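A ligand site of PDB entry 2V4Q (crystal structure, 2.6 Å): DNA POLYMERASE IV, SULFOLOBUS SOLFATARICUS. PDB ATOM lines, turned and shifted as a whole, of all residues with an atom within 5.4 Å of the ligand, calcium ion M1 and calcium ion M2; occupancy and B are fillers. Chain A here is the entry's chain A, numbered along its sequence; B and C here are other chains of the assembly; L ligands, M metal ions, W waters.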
ATOM      1  N   ASP A  13       5.613   7.497  -6.466  1.00  0.00           N
ATOM      2  CA  ASP A  13       5.119   6.641  -7.529  1.00  0.00           C
ATOM      3  C   ASP A  13       6.289   6.109  -8.396  1.00  0.00           C
ATOM      4  O   ASP A  13       6.976   6.883  -9.068  1.00  0.00           O
ATOM      5  CB  ASP A  13       4.125   7.487  -8.328  1.00  0.00           C
ATOM      6  CG  ASP A  13       3.819   6.933  -9.674  1.00  0.00           C
ATOM      7  OD1 ASP A  13       4.726   6.990 -10.533  1.00  0.00           O
ATOM      8  OD2 ASP A  13       2.664   6.467  -9.866  1.00  0.00           O
ATOM      9  N   PHE A  14       6.505   4.797  -8.383  1.00  0.00           N
ATOM     10  CA  PHE A  14       7.619   4.174  -9.103  1.00  0.00           C
ATOM     11  C   PHE A  14       7.472   4.268 -10.616  1.00  0.00           C
ATOM     12  O   PHE A  14       6.437   3.987 -11.137  1.00  0.00           O
ATOM     13  CB  PHE A  14       7.749   2.692  -8.728  1.00  0.00           C
ATOM     14  CG  PHE A  14       7.500   2.403  -7.278  1.00  0.00           C
ATOM     15  CD1 PHE A  14       7.658   3.366  -6.308  1.00  0.00           C
ATOM     16  CD2 PHE A  14       7.119   1.127  -6.871  1.00  0.00           C
ATOM     17  CE1 PHE A  14       7.447   3.085  -4.954  1.00  0.00           C
ATOM     18  CE2 PHE A  14       6.902   0.833  -5.517  1.00  0.00           C
ATOM     19  CZ  PHE A  14       7.068   1.831  -4.557  1.00  0.00           C
ATOM     20  N   ASP A  15       8.543   4.622 -11.320  1.00  0.00           N
ATOM     21  CA  ASP A  15       8.448   4.765 -12.765  1.00  0.00           C
ATOM     22  C   ASP A  15       8.323   3.463 -13.555  1.00  0.00           C
ATOM     23  O   ASP A  15       9.069   2.507 -13.332  1.00  0.00           O
ATOM     24  CB  ASP A  15       9.638   5.575 -13.277  1.00  0.00           C
ATOM     25  CG  ASP A  15       9.800   6.912 -12.522  1.00  0.00           C
ATOM     26  OD1 ASP A  15       8.778   7.476 -12.081  1.00  0.00           O
ATOM     27  OD2 ASP A  15      10.941   7.398 -12.378  1.00  0.00           O
ATOM     28  N   TYR A  16       7.381   3.471 -14.511  1.00  0.00           N
ATOM     29  CA  TYR A  16       7.077   2.333 -15.367  1.00  0.00           C
ATOM     30  C   TYR A  16       7.433   1.047 -14.683  1.00  0.00           C
ATOM     31  O   TYR A  16       8.016   0.149 -15.247  1.00  0.00           O
ATOM     32  CB  TYR A  16       7.798   2.473 -16.717  1.00  0.00           C
ATOM     33  CG  TYR A  16       9.288   2.611 -16.643  1.00  0.00           C
ATOM     34  CD1 TYR A  16      10.112   1.498 -16.740  1.00  0.00           C
ATOM     35  CD2 TYR A  16       9.884   3.855 -16.488  1.00  0.00           C
ATOM     36  CE1 TYR A  16      11.480   1.617 -16.669  1.00  0.00           C
ATOM     37  CE2 TYR A  16      11.273   3.995 -16.416  1.00  0.00           C
ATOM     38  CZ  TYR A  16      12.068   2.865 -16.517  1.00  0.00           C
ATOM     39  OH  TYR A  16      13.440   2.974 -16.436  1.00  0.00           O
ATOM     40  N   PHE A  17       7.005   0.994 -13.439  1.00  0.00           N
ATOM     41  CA  PHE A  17       7.284  -0.086 -12.534  1.00  0.00           C
ATOM     42  C   PHE A  17       7.534  -1.480 -13.032  1.00  0.00           C
ATOM     43  O   PHE A  17       8.659  -1.955 -12.859  1.00  0.00           O
ATOM     44  CB  PHE A  17       6.239  -0.127 -11.440  1.00  0.00           C
ATOM     45  CG  PHE A  17       6.666  -0.927 -10.250  1.00  0.00           C
ATOM     46  CD1 PHE A  17       7.949  -0.851  -9.805  1.00  0.00           C
ATOM     47  CD2 PHE A  17       5.794  -1.727  -9.570  1.00  0.00           C
ATOM     48  CE1 PHE A  17       8.354  -1.550  -8.704  1.00  0.00           C
ATOM     49  CE2 PHE A  17       6.191  -2.437  -8.455  1.00  0.00           C
ATOM     50  CZ  PHE A  17       7.473  -2.346  -8.026  1.00  0.00           C
ATOM     51  N   TYR A  18       6.549  -2.159 -13.616  1.00  0.00           N
ATOM     52  CA  TYR A  18       6.809  -3.531 -14.064  1.00  0.00           C
ATOM     53  C   TYR A  18       7.991  -3.616 -15.032  1.00  0.00           C
ATOM     54  O   TYR A  18       8.894  -4.454 -14.849  1.00  0.00           O
ATOM     55  CB  TYR A  18       5.589  -4.161 -14.708  1.00  0.00           C
ATOM     56  CG  TYR A  18       4.459  -4.418 -13.745  1.00  0.00           C
ATOM     57  CD1 TYR A  18       4.459  -3.828 -12.470  1.00  0.00           C
ATOM     58  CD2 TYR A  18       3.373  -5.211 -14.128  1.00  0.00           C
ATOM     59  CE1 TYR A  18       3.387  -4.022 -11.577  1.00  0.00           C
ATOM     60  CE2 TYR A  18       2.297  -5.420 -13.248  1.00  0.00           C
ATOM     61  CZ  TYR A  18       2.316  -4.816 -11.979  1.00  0.00           C
ATOM     62  OH  TYR A  18       1.256  -4.970 -11.104  1.00  0.00           O
ATOM     63  N   ALA A  19       8.026  -2.758 -16.042  1.00  0.00           N
ATOM     64  CA  ALA A  19       9.120  -2.846 -16.981  1.00  0.00           C
ATOM     65  C   ALA A  19      10.416  -2.480 -16.282  1.00  0.00           C
ATOM     66  O   ALA A  19      11.456  -3.105 -16.494  1.00  0.00           O
ATOM     67  CB  ALA A  19       8.872  -1.927 -18.156  1.00  0.00           C
ATOM     68  N   VAL A  38       0.885  -9.640 -21.140  1.00  0.00           N
ATOM     69  CA  VAL A  38      -0.001 -10.626 -20.539  1.00  0.00           C
ATOM     70  C   VAL A  38      -0.571 -11.412 -21.718  1.00  0.00           C
ATOM     71  O   VAL A  38      -1.543 -10.979 -22.344  1.00  0.00           O
ATOM     72  CB  VAL A  38      -1.147  -9.907 -19.779  1.00  0.00           C
ATOM     73  CG1 VAL A  38      -2.109 -10.920 -19.201  1.00  0.00           C
ATOM     74  CG2 VAL A  38      -0.594  -9.054 -18.683  1.00  0.00           C
ATOM     75  N   VAL A  49      -0.752  -5.320 -23.395  1.00  0.00           N
ATOM     76  CA  VAL A  49       0.434  -4.770 -22.774  1.00  0.00           C
ATOM     77  C   VAL A  49       0.174  -4.414 -21.303  1.00  0.00           C
ATOM     78  O   VAL A  49      -0.719  -3.619 -20.987  1.00  0.00           O
ATOM     79  CB  VAL A  49       0.918  -3.490 -23.519  1.00  0.00           C
ATOM     80  CG1 VAL A  49       2.054  -2.829 -22.748  1.00  0.00           C
ATOM     81  CG2 VAL A  49       1.363  -3.832 -24.925  1.00  0.00           C
ATOM     82  N   ALA A  50       0.936  -5.006 -20.395  1.00  0.00           N
ATOM     83  CA  ALA A  50       0.775  -4.661 -18.985  1.00  0.00           C
ATOM     84  C   ALA A  50       1.209  -3.205 -18.864  1.00  0.00           C
ATOM     85  O   ALA A  50       0.471  -2.354 -18.414  1.00  0.00           O
ATOM     86  CB  ALA A  50       1.660  -5.537 -18.120  1.00  0.00           C
ATOM     87  N   THR A  51       2.446  -2.950 -19.267  1.00  0.00           N
ATOM     88  CA  THR A  51       3.020  -1.621 -19.229  1.00  0.00           C
ATOM     89  C   THR A  51       4.277  -1.697 -20.062  1.00  0.00           C
ATOM     90  O   THR A  51       4.652  -2.778 -20.501  1.00  0.00           O
ATOM     91  CB  THR A  51       3.376  -1.208 -17.806  1.00  0.00           C
ATOM     92  OG1 THR A  51       3.650   0.198 -17.778  1.00  0.00           O
ATOM     93  CG2 THR A  51       4.603  -1.986 -17.330  1.00  0.00           C
ATOM     94  N   TYR A  54       9.610   3.847 -20.937  1.00  0.00           N
ATOM     95  CA  TYR A  54       9.492   5.033 -21.778  1.00  0.00           C
ATOM     96  C   TYR A  54      10.044   4.891 -23.178  1.00  0.00           C
ATOM     97  O   TYR A  54       9.481   5.463 -24.107  1.00  0.00           O
ATOM     98  CB  TYR A  54      10.101   6.234 -21.081  1.00  0.00           C
ATOM     99  CG  TYR A  54       9.260   6.696 -19.917  1.00  0.00           C
ATOM    100  CD1 TYR A  54       9.577   6.319 -18.599  1.00  0.00           C
ATOM    101  CD2 TYR A  54       8.102   7.438 -20.131  1.00  0.00           C
ATOM    102  CE1 TYR A  54       8.750   6.667 -17.541  1.00  0.00           C
ATOM    103  CE2 TYR A  54       7.268   7.797 -19.068  1.00  0.00           C
ATOM    104  CZ  TYR A  54       7.610   7.406 -17.787  1.00  0.00           C
ATOM    105  OH  TYR A  54       6.801   7.745 -16.725  1.00  0.00           O
ATOM    106  N   ARG A  57       7.123   3.787 -24.705  1.00  0.00           N
ATOM    107  CA  ARG A  57       5.955   4.653 -24.568  1.00  0.00           C
ATOM    108  C   ARG A  57       5.950   5.856 -25.522  1.00  0.00           C
ATOM    109  O   ARG A  57       4.886   6.312 -25.950  1.00  0.00           O
ATOM    110  CB  ARG A  57       5.809   5.126 -23.107  1.00  0.00           C
ATOM    111  CG  ARG A  57       5.289   4.031 -22.162  1.00  0.00           C
ATOM    112  CD  ARG A  57       3.915   4.371 -21.644  1.00  0.00           C
ATOM    113  NE  ARG A  57       3.994   5.201 -20.459  1.00  0.00           N
ATOM    114  CZ  ARG A  57       4.451   4.788 -19.279  1.00  0.00           C
ATOM    115  NH1 ARG A  57       4.877   3.536 -19.122  1.00  0.00           N
ATOM    116  NH2 ARG A  57       4.484   5.610 -18.254  1.00  0.00           N
ATOM    117  N   ALA A  63      -0.119   1.009 -21.790  1.00  0.00           N
ATOM    118  CA  ALA A  63      -0.855  -0.082 -21.178  1.00  0.00           C
ATOM    119  C   ALA A  63      -2.257  -0.208 -21.746  1.00  0.00           C
ATOM    120  O   ALA A  63      -2.966   0.782 -21.866  1.00  0.00           O
ATOM    121  CB  ALA A  63      -0.913   0.130 -19.654  1.00  0.00           C
ATOM    122  N   GLY A  64      -2.644  -1.424 -22.114  1.00  0.00           N
ATOM    123  CA  GLY A  64      -3.977  -1.621 -22.640  1.00  0.00           C
ATOM    124  C   GLY A  64      -4.094  -2.090 -24.087  1.00  0.00           C
ATOM    125  O   GLY A  64      -4.969  -2.896 -24.382  1.00  0.00           O
ATOM    126  N   MET A  82       4.521 -10.867 -18.101  1.00  0.00           N
ATOM    127  CA  MET A  82       4.353 -10.232 -16.796  1.00  0.00           C
ATOM    128  C   MET A  82       4.527 -11.217 -15.632  1.00  0.00           C
ATOM    129  O   MET A  82       4.018 -12.326 -15.688  1.00  0.00           O
ATOM    130  CB  MET A  82       2.971  -9.603 -16.714  1.00  0.00           C
ATOM    131  CG  MET A  82       2.679  -8.985 -15.398  1.00  0.00           C
ATOM    132  SD  MET A  82       0.949  -8.495 -15.379  1.00  0.00           S
ATOM    133  CE  MET A  82       0.254  -9.924 -14.470  1.00  0.00           C
ATOM    134  N   SER A 109      -1.624   1.710  -3.899  1.00  0.00           N
ATOM    135  CA  SER A 109      -1.584   0.678  -4.943  1.00  0.00           C
ATOM    136  C   SER A 109      -0.252  -0.071  -4.909  1.00  0.00           C
ATOM    137  O   SER A 109       0.617   0.204  -4.075  1.00  0.00           O
ATOM    138  CB  SER A 109      -1.769   1.294  -6.335  1.00  0.00           C
ATOM    139  OG  SER A 109      -0.531   1.724  -6.869  1.00  0.00           O
ATOM    140  N   ILE A 110      -0.095  -0.998  -5.845  1.00  0.00           N
ATOM    141  CA  ILE A 110       1.125  -1.798  -5.874  1.00  0.00           C
ATOM    142  C   ILE A 110       2.375  -0.966  -6.111  1.00  0.00           C
ATOM    143  O   ILE A 110       3.498  -1.473  -5.992  1.00  0.00           O
ATOM    144  CB  ILE A 110       1.105  -2.914  -6.974  1.00  0.00           C
ATOM    145  CG1 ILE A 110       2.219  -3.931  -6.703  1.00  0.00           C
ATOM    146  CG2 ILE A 110       1.312  -2.286  -8.374  1.00  0.00           C
ATOM    147  CD1 ILE A 110       2.372  -4.949  -7.765  1.00  0.00           C
ATOM    148  N   ASP A 111       2.216   0.303  -6.457  1.00  0.00           N
ATOM    149  CA  ASP A 111       3.424   1.070  -6.700  1.00  0.00           C
ATOM    150  C   ASP A 111       3.362   2.562  -6.321  1.00  0.00           C
ATOM    151  O   ASP A 111       4.087   3.369  -6.890  1.00  0.00           O
ATOM    152  CB  ASP A 111       3.774   0.977  -8.155  1.00  0.00           C
ATOM    153  CG  ASP A 111       2.915   1.890  -8.962  1.00  0.00           C
ATOM    154  OD1 ASP A 111       1.716   2.008  -8.631  1.00  0.00           O
ATOM    155  OD2 ASP A 111       3.423   2.509  -9.912  1.00  0.00           O
ATOM    156  N   GLU A 112       2.488   2.934  -5.397  1.00  0.00           N
ATOM    157  CA  GLU A 112       2.422   4.335  -4.992  1.00  0.00           C
ATOM    158  C   GLU A 112       1.956   4.437  -3.558  1.00  0.00           C
ATOM    159  O   GLU A 112       1.211   3.587  -3.088  1.00  0.00           O
ATOM    160  CB  GLU A 112       1.498   5.125  -5.917  1.00  0.00           C
ATOM    161  CG  GLU A 112       0.063   4.705  -5.880  1.00  0.00           C
ATOM    162  CD  GLU A 112      -0.655   5.036  -7.181  1.00  0.00           C
ATOM    163  OE1 GLU A 112      -0.720   6.217  -7.578  1.00  0.00           O
ATOM    164  OE2 GLU A 112      -1.158   4.100  -7.837  1.00  0.00           O
ATOM    165  N   LYS A 165       6.670  13.445 -13.721  1.00  0.00           N
ATOM    166  CA  LYS A 165       7.083  12.180 -14.316  1.00  0.00           C
ATOM    167  C   LYS A 165       7.893  12.407 -15.576  1.00  0.00           C
ATOM    168  O   LYS A 165       7.566  13.295 -16.377  1.00  0.00           O
ATOM    169  CB  LYS A 165       5.858  11.322 -14.678  1.00  0.00           C
ATOM    170  CG  LYS A 165       5.195  10.641 -13.479  1.00  0.00           C
ATOM    171  CD  LYS A 165       4.058   9.712 -13.925  1.00  0.00           C
ATOM    172  CE  LYS A 165       3.384   9.037 -12.714  1.00  0.00           C
ATOM    173  NZ  LYS A 165       2.202   8.222 -13.074  1.00  0.00           N
ATOM    174  N   PRO A 166       8.960  11.603 -15.782  1.00  0.00           N
ATOM    175  CA  PRO A 166       9.390  10.527 -14.881  1.00  0.00           C
ATOM    176  C   PRO A 166      10.593  10.937 -14.037  1.00  0.00           C
ATOM    177  O   PRO A 166      11.182  11.995 -14.235  1.00  0.00           O
ATOM    178  CB  PRO A 166       9.730   9.406 -15.840  1.00  0.00           C
ATOM    179  CG  PRO A 166      10.447  10.170 -16.904  1.00  0.00           C
ATOM    180  CD  PRO A 166       9.601  11.429 -17.097  1.00  0.00           C
ATOM    181  P    DC B   4      -8.154  -9.411 -23.487  1.00  0.00           P
ATOM    182  OP1  DC B   4      -8.127 -10.587 -24.384  1.00  0.00           O
ATOM    183  OP2  DC B   4      -9.442  -8.962 -22.918  1.00  0.00           O
ATOM    184  O5'  DC B   4      -7.123  -9.735 -22.301  1.00  0.00           O
ATOM    185  C5'  DC B   4      -5.952 -10.475 -22.577  1.00  0.00           C
ATOM    186  C4'  DC B   4      -5.107 -10.563 -21.324  1.00  0.00           C
ATOM    187  O4'  DC B   4      -4.525  -9.281 -21.025  1.00  0.00           O
ATOM    188  C3'  DC B   4      -5.900 -10.949 -20.076  1.00  0.00           C
ATOM    189  O3'  DC B   4      -5.120 -11.774 -19.236  1.00  0.00           O
ATOM    190  C2'  DC B   4      -6.199  -9.625 -19.411  1.00  0.00           C
ATOM    191  C1'  DC B   4      -4.946  -8.831 -19.745  1.00  0.00           C
ATOM    192  N1   DC B   4      -5.129  -7.363 -19.817  1.00  0.00           N
ATOM    193  C2   DC B   4      -4.302  -6.551 -19.060  1.00  0.00           C
ATOM    194  O2   DC B   4      -3.415  -7.081 -18.364  1.00  0.00           O
ATOM    195  N3   DC B   4      -4.470  -5.215 -19.084  1.00  0.00           N
ATOM    196  C4   DC B   4      -5.414  -4.668 -19.843  1.00  0.00           C
ATOM    197  N4   DC B   4      -5.531  -3.347 -19.819  1.00  0.00           N
ATOM    198  C5   DC B   4      -6.276  -5.482 -20.648  1.00  0.00           C
ATOM    199  C6   DC B   4      -6.099  -6.813 -20.603  1.00  0.00           C
ATOM    200  P   M1G B   5      -5.808 -12.521 -18.018  1.00  0.00           P
ATOM    201  OP1 M1G B   5      -5.087 -13.785 -17.737  1.00  0.00           O
ATOM    202  OP2 M1G B   5      -7.257 -12.539 -18.311  1.00  0.00           O
ATOM    203  O5' M1G B   5      -5.555 -11.468 -16.826  1.00  0.00           O
ATOM    204  C5' M1G B   5      -4.239 -11.262 -16.305  1.00  0.00           C
ATOM    205  C4' M1G B   5      -4.250 -10.052 -15.360  1.00  0.00           C
ATOM    206  O4' M1G B   5      -4.675  -8.866 -16.050  1.00  0.00           O
ATOM    207  C3' M1G B   5      -5.339 -10.334 -14.335  1.00  0.00           C
ATOM    208  O3' M1G B   5      -4.730 -10.478 -13.056  1.00  0.00           O
ATOM    209  C2' M1G B   5      -6.242  -9.103 -14.389  1.00  0.00           C
ATOM    210  C1' M1G B   5      -5.325  -8.079 -15.041  1.00  0.00           C
ATOM    211  N9  M1G B   5      -6.102  -6.985 -15.678  1.00  0.00           N
ATOM    212  C8  M1G B   5      -7.027  -7.151 -16.629  1.00  0.00           C
ATOM    213  N7  M1G B   5      -7.441  -5.949 -17.038  1.00  0.00           N
ATOM    214  C5  M1G B   5      -6.786  -5.031 -16.346  1.00  0.00           C
ATOM    215  C6  M1G B   5      -6.831  -3.636 -16.335  1.00  0.00           C
ATOM    216  O6  M1G B   5      -7.569  -3.017 -17.098  1.00  0.00           O
ATOM    217  N1  M1G B   5      -6.021  -2.949 -15.420  1.00  0.00           N
ATOM    218  C2  M1G B   5      -5.188  -3.673 -14.555  1.00  0.00           C
ATOM    219  N2  M1G B   5      -4.427  -3.027 -13.658  1.00  0.00           N
ATOM    220  N3  M1G B   5      -5.163  -5.013 -14.606  1.00  0.00           N
ATOM    221  C4  M1G B   5      -5.937  -5.692 -15.465  1.00  0.00           C
ATOM    222  C6A M1G B   5      -4.462  -1.711 -13.562  1.00  0.00           C
ATOM    223  C7A M1G B   5      -5.274  -0.940 -14.379  1.00  0.00           C
ATOM    224  C8A M1G B   5      -6.076  -1.562 -15.337  1.00  0.00           C
ATOM    225  P    DC C  13      -8.577   8.121 -13.351  1.00  0.00           P
ATOM    226  OP1  DC C  13      -8.223   9.448 -12.807  1.00  0.00           O
ATOM    227  OP2  DC C  13      -8.764   7.946 -14.813  1.00  0.00           O
ATOM    228  O5'  DC C  13      -7.458   7.090 -12.838  1.00  0.00           O
ATOM    229  C5'  DC C  13      -7.420   6.624 -11.476  1.00  0.00           C
ATOM    230  C4'  DC C  13      -6.408   5.516 -11.347  1.00  0.00           C
ATOM    231  O4'  DC C  13      -7.056   4.203 -11.473  1.00  0.00           O
ATOM    232  C3'  DC C  13      -5.363   5.556 -12.441  1.00  0.00           C
ATOM    233  O3'  DC C  13      -4.075   5.302 -11.923  1.00  0.00           O
ATOM    234  C2'  DC C  13      -5.775   4.498 -13.399  1.00  0.00           C
ATOM    235  C1'  DC C  13      -6.331   3.468 -12.454  1.00  0.00           C
ATOM    236  N1   DC C  13      -7.225   2.475 -13.053  1.00  0.00           N
ATOM    237  C2   DC C  13      -7.375   1.255 -12.398  1.00  0.00           C
ATOM    238  O2   DC C  13      -6.784   1.071 -11.326  1.00  0.00           O
ATOM    239  N3   DC C  13      -8.133   0.293 -12.935  1.00  0.00           N
ATOM    240  C4   DC C  13      -8.756   0.513 -14.096  1.00  0.00           C
ATOM    241  N4   DC C  13      -9.471  -0.502 -14.633  1.00  0.00           N
ATOM    242  C5   DC C  13      -8.670   1.779 -14.768  1.00  0.00           C
ATOM    243  C6   DC C  13      -7.899   2.728 -14.220  1.00  0.00           C
ATOM    244  P    DC C  14      -3.058   6.499 -11.720  1.00  0.00           P
ATOM    245  OP1  DC C  14      -3.824   7.683 -12.171  1.00  0.00           O
ATOM    246  OP2  DC C  14      -1.757   6.167 -12.346  1.00  0.00           O
ATOM    247  O5'  DC C  14      -2.950   6.649 -10.116  1.00  0.00           O
ATOM    248  C5'  DC C  14      -3.694   5.802  -9.256  1.00  0.00           C
ATOM    249  C4'  DC C  14      -4.211   6.571  -8.070  1.00  0.00           C
ATOM    250  O4'  DC C  14      -5.530   7.104  -8.370  1.00  0.00           O
ATOM    251  C3'  DC C  14      -4.339   5.764  -6.800  1.00  0.00           C
ATOM    252  O3'  DC C  14      -3.506   6.336  -5.736  1.00  0.00           O
ATOM    253  C2'  DC C  14      -5.812   5.788  -6.466  1.00  0.00           C
ATOM    254  C1'  DC C  14      -6.353   7.013  -7.210  1.00  0.00           C
ATOM    255  N1   DC C  14      -7.754   6.846  -7.628  1.00  0.00           N
ATOM    256  C2   DC C  14      -8.623   7.913  -7.481  1.00  0.00           C
ATOM    257  O2   DC C  14      -8.186   8.995  -7.072  1.00  0.00           O
ATOM    258  N3   DC C  14      -9.931   7.753  -7.797  1.00  0.00           N
ATOM    259  C4   DC C  14     -10.368   6.573  -8.265  1.00  0.00           C
ATOM    260  N4   DC C  14     -11.668   6.451  -8.534  1.00  0.00           N
ATOM    261  C5   DC C  14      -9.488   5.484  -8.451  1.00  0.00           C
ATOM    262  C6   DC C  14      -8.205   5.664  -8.135  1.00  0.00           C
HETATM  263  P1  LIG L   1       4.266   5.757 -14.962  1.00  0.00           P
HETATM  264  O1  LIG L   1       3.791   6.788 -16.103  1.00  0.00           O
HETATM  265  O2  LIG L   1       5.816   6.080 -14.670  1.00  0.00           O
HETATM  266  O3  LIG L   1       3.425   5.843 -13.748  1.00  0.00           O
HETATM  267  O4  LIG L   1       4.257   4.286 -15.630  1.00  0.00           O
HETATM  268  P2  LIG L   1       3.732   3.041 -14.731  1.00  0.00           P
HETATM  269  O5  LIG L   1       3.870   1.740 -15.434  1.00  0.00           O
HETATM  270  O6  LIG L   1       4.312   3.065 -13.371  1.00  0.00           O
HETATM  271  O7  LIG L   1       2.126   3.181 -14.652  1.00  0.00           O
HETATM  272  P3  LIG L   1       1.315   3.230 -13.256  1.00  0.00           P
HETATM  273  O8  LIG L   1      -0.094   3.864 -13.686  1.00  0.00           O
HETATM  274  O9  LIG L   1       1.947   3.989 -12.157  1.00  0.00           O
HETATM  275  O10 LIG L   1       1.020   1.679 -12.907  1.00  0.00           O
HETATM  276  C1  LIG L   1       1.951   0.927 -12.130  1.00  0.00           C
HETATM  277  C2  LIG L   1       1.801  -0.535 -12.556  1.00  0.00           C
HETATM  278  O11 LIG L   1       0.401  -0.846 -12.694  1.00  0.00           O
HETATM  279  C3  LIG L   1       2.317  -0.739 -13.983  1.00  0.00           C
HETATM  280  O12 LIG L   1       3.739  -0.863 -13.965  1.00  0.00           O
HETATM  281  C4  LIG L   1       1.711  -2.117 -14.229  1.00  0.00           C
HETATM  282  C5  LIG L   1       0.323  -1.963 -13.595  1.00  0.00           C
HETATM  283  N1  LIG L   1      -0.679  -1.630 -14.647  1.00  0.00           N
HETATM  284  C6  LIG L   1      -1.089  -0.403 -14.978  1.00  0.00           C
HETATM  285  N2  LIG L   1      -2.013  -0.499 -15.932  1.00  0.00           N
HETATM  286  C7  LIG L   1      -2.204  -1.783 -16.208  1.00  0.00           C
HETATM  287  C8  LIG L   1      -3.036  -2.457 -17.099  1.00  0.00           C
HETATM  288  O13 LIG L   1      -3.785  -1.832 -17.850  1.00  0.00           O
HETATM  289  N3  LIG L   1      -2.971  -3.857 -17.157  1.00  0.00           N
HETATM  290  C9  LIG L   1      -2.090  -4.533 -16.298  1.00  0.00           C
HETATM  291  N4  LIG L   1      -2.001  -5.864 -16.317  1.00  0.00           N
HETATM  292  N5  LIG L   1      -1.315  -3.848 -15.432  1.00  0.00           N
HETATM  293  C10 LIG L   1      -1.354  -2.517 -15.382  1.00  0.00           C
HETATM  294 CA    CA M   1       4.011   4.547 -11.396  1.00  0.00          CA
HETATM  295 CA    CA M   2       1.037   4.324  -9.744  1.00  0.00          CA
HETATM  296  O   HOH W   1      -3.174   1.576 -16.835  1.00  0.00           O
HETATM  297  O   HOH W   2      -0.219   6.030 -10.759  1.00  0.00           O
HETATM  298  O   HOH W   3      -5.081   0.677 -18.493  1.00  0.00           O
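N1 of M1G 5 of chain B sits close to O13 of the ligand, 3.5 Å away.
OP2 of DC 14 of chain C lies close to an oxygen (O8) of the ligand.
CA of Asp 15 touches O2 of the ligand, at 3.5 Å.
Ala 50 touches the ligand (O to C7, 3.5 Å).
CB of Ala 63 touches O13 of the ligand (3.9 Å).
Hydrophobic or aromatic side chains that line the ligand: Phe 17, Tyr 18, Tyr 54 and Ala 63.
Along chain A the residues within 4 Å of the ligand span positions 13 to 165.
Of the 26 residues printed, 3 come within 4 Å of calcium ion M1.
O1 of the ligand lies within salt-bridge range of NH2 of Arg 57 (2.5 Å).
NZ of Lys 165 is in salt-bridge range of O1 of the ligand, at 3.7 Å.
O2 of DC 4 of chain B lies within hydrogen-bond range of a nitrogen (N4) of the ligand, 2.8 Å away.
The side-chain hydroxyl (OG1) of Thr 51 lies within hydrogen-bond range of an oxygen (O5) of the ligand, at 2.8 Å.
OH of Tyr 54 sits at hydrogen-bond distance from O2 of the ligand (2.8 Å).
O2 of the ligand is in hydrogen-bond range of N of Tyr 16 (3.0 Å).
The backbone NH (N) of Tyr 18 sits at hydrogen-bond distance from an oxygen (O12) of the ligand (3.1 Å).
N of Phe 17 lies close to O6 of the ligand, at 3.4 Å.
Calcium ion M1 is bound by O9 of the ligand (2.3 Å), O6 of the ligand (2.5 Å), O of Phe 14 of chain A (2.5 Å), OD2 of Asp 111 (2.6 Å), OD1 of Asp 13 of chain A (2.7 Å), O3 of the ligand (2.7 Å) and OD2 of Asp 13 of chain A (2.8 Å).
Within 4 Å of calcium ion M2: Asp 13 of chain A, Asp 111 and Glu 112.
The nearest printed residue that does not touch calcium ion M2 is Ser 109 (4.2 Å).
Water W2 bridges O5' of DC 14 of chain C and the side-chain carboxylate (OE1) of Glu 112.
Calcium ion M2 is bound by water W2 (2.3 Å).
O9 of the ligand is bound to calcium ion M2.
The side-chain carboxylate (OD1) of Asp 111 binds calcium ion M2, at 2.7 Å.
The side-chain carboxylate (OD2) of Asp 13 of chain A binds calcium ion M2, at 2.7 Å.
Calcium ion M2 is bound by the side-chain carboxylate (OE2) of Glu 112, at 2.9 Å.
Slightly farther from calcium ion M2 lies OD2 of Asp 111 (3.0 Å).
N of Asp 111 sits close to OG of Ser 109, 3.1 Å away.
The side-chain carboxylate of Asp 13 of chain A lies close to the side-chain amino group of Lys 165.
The side-chain hydroxyl (OG) of Ser 109 lies close to the side-chain carboxylate (OE2) of Glu 112 (2.6 Å).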
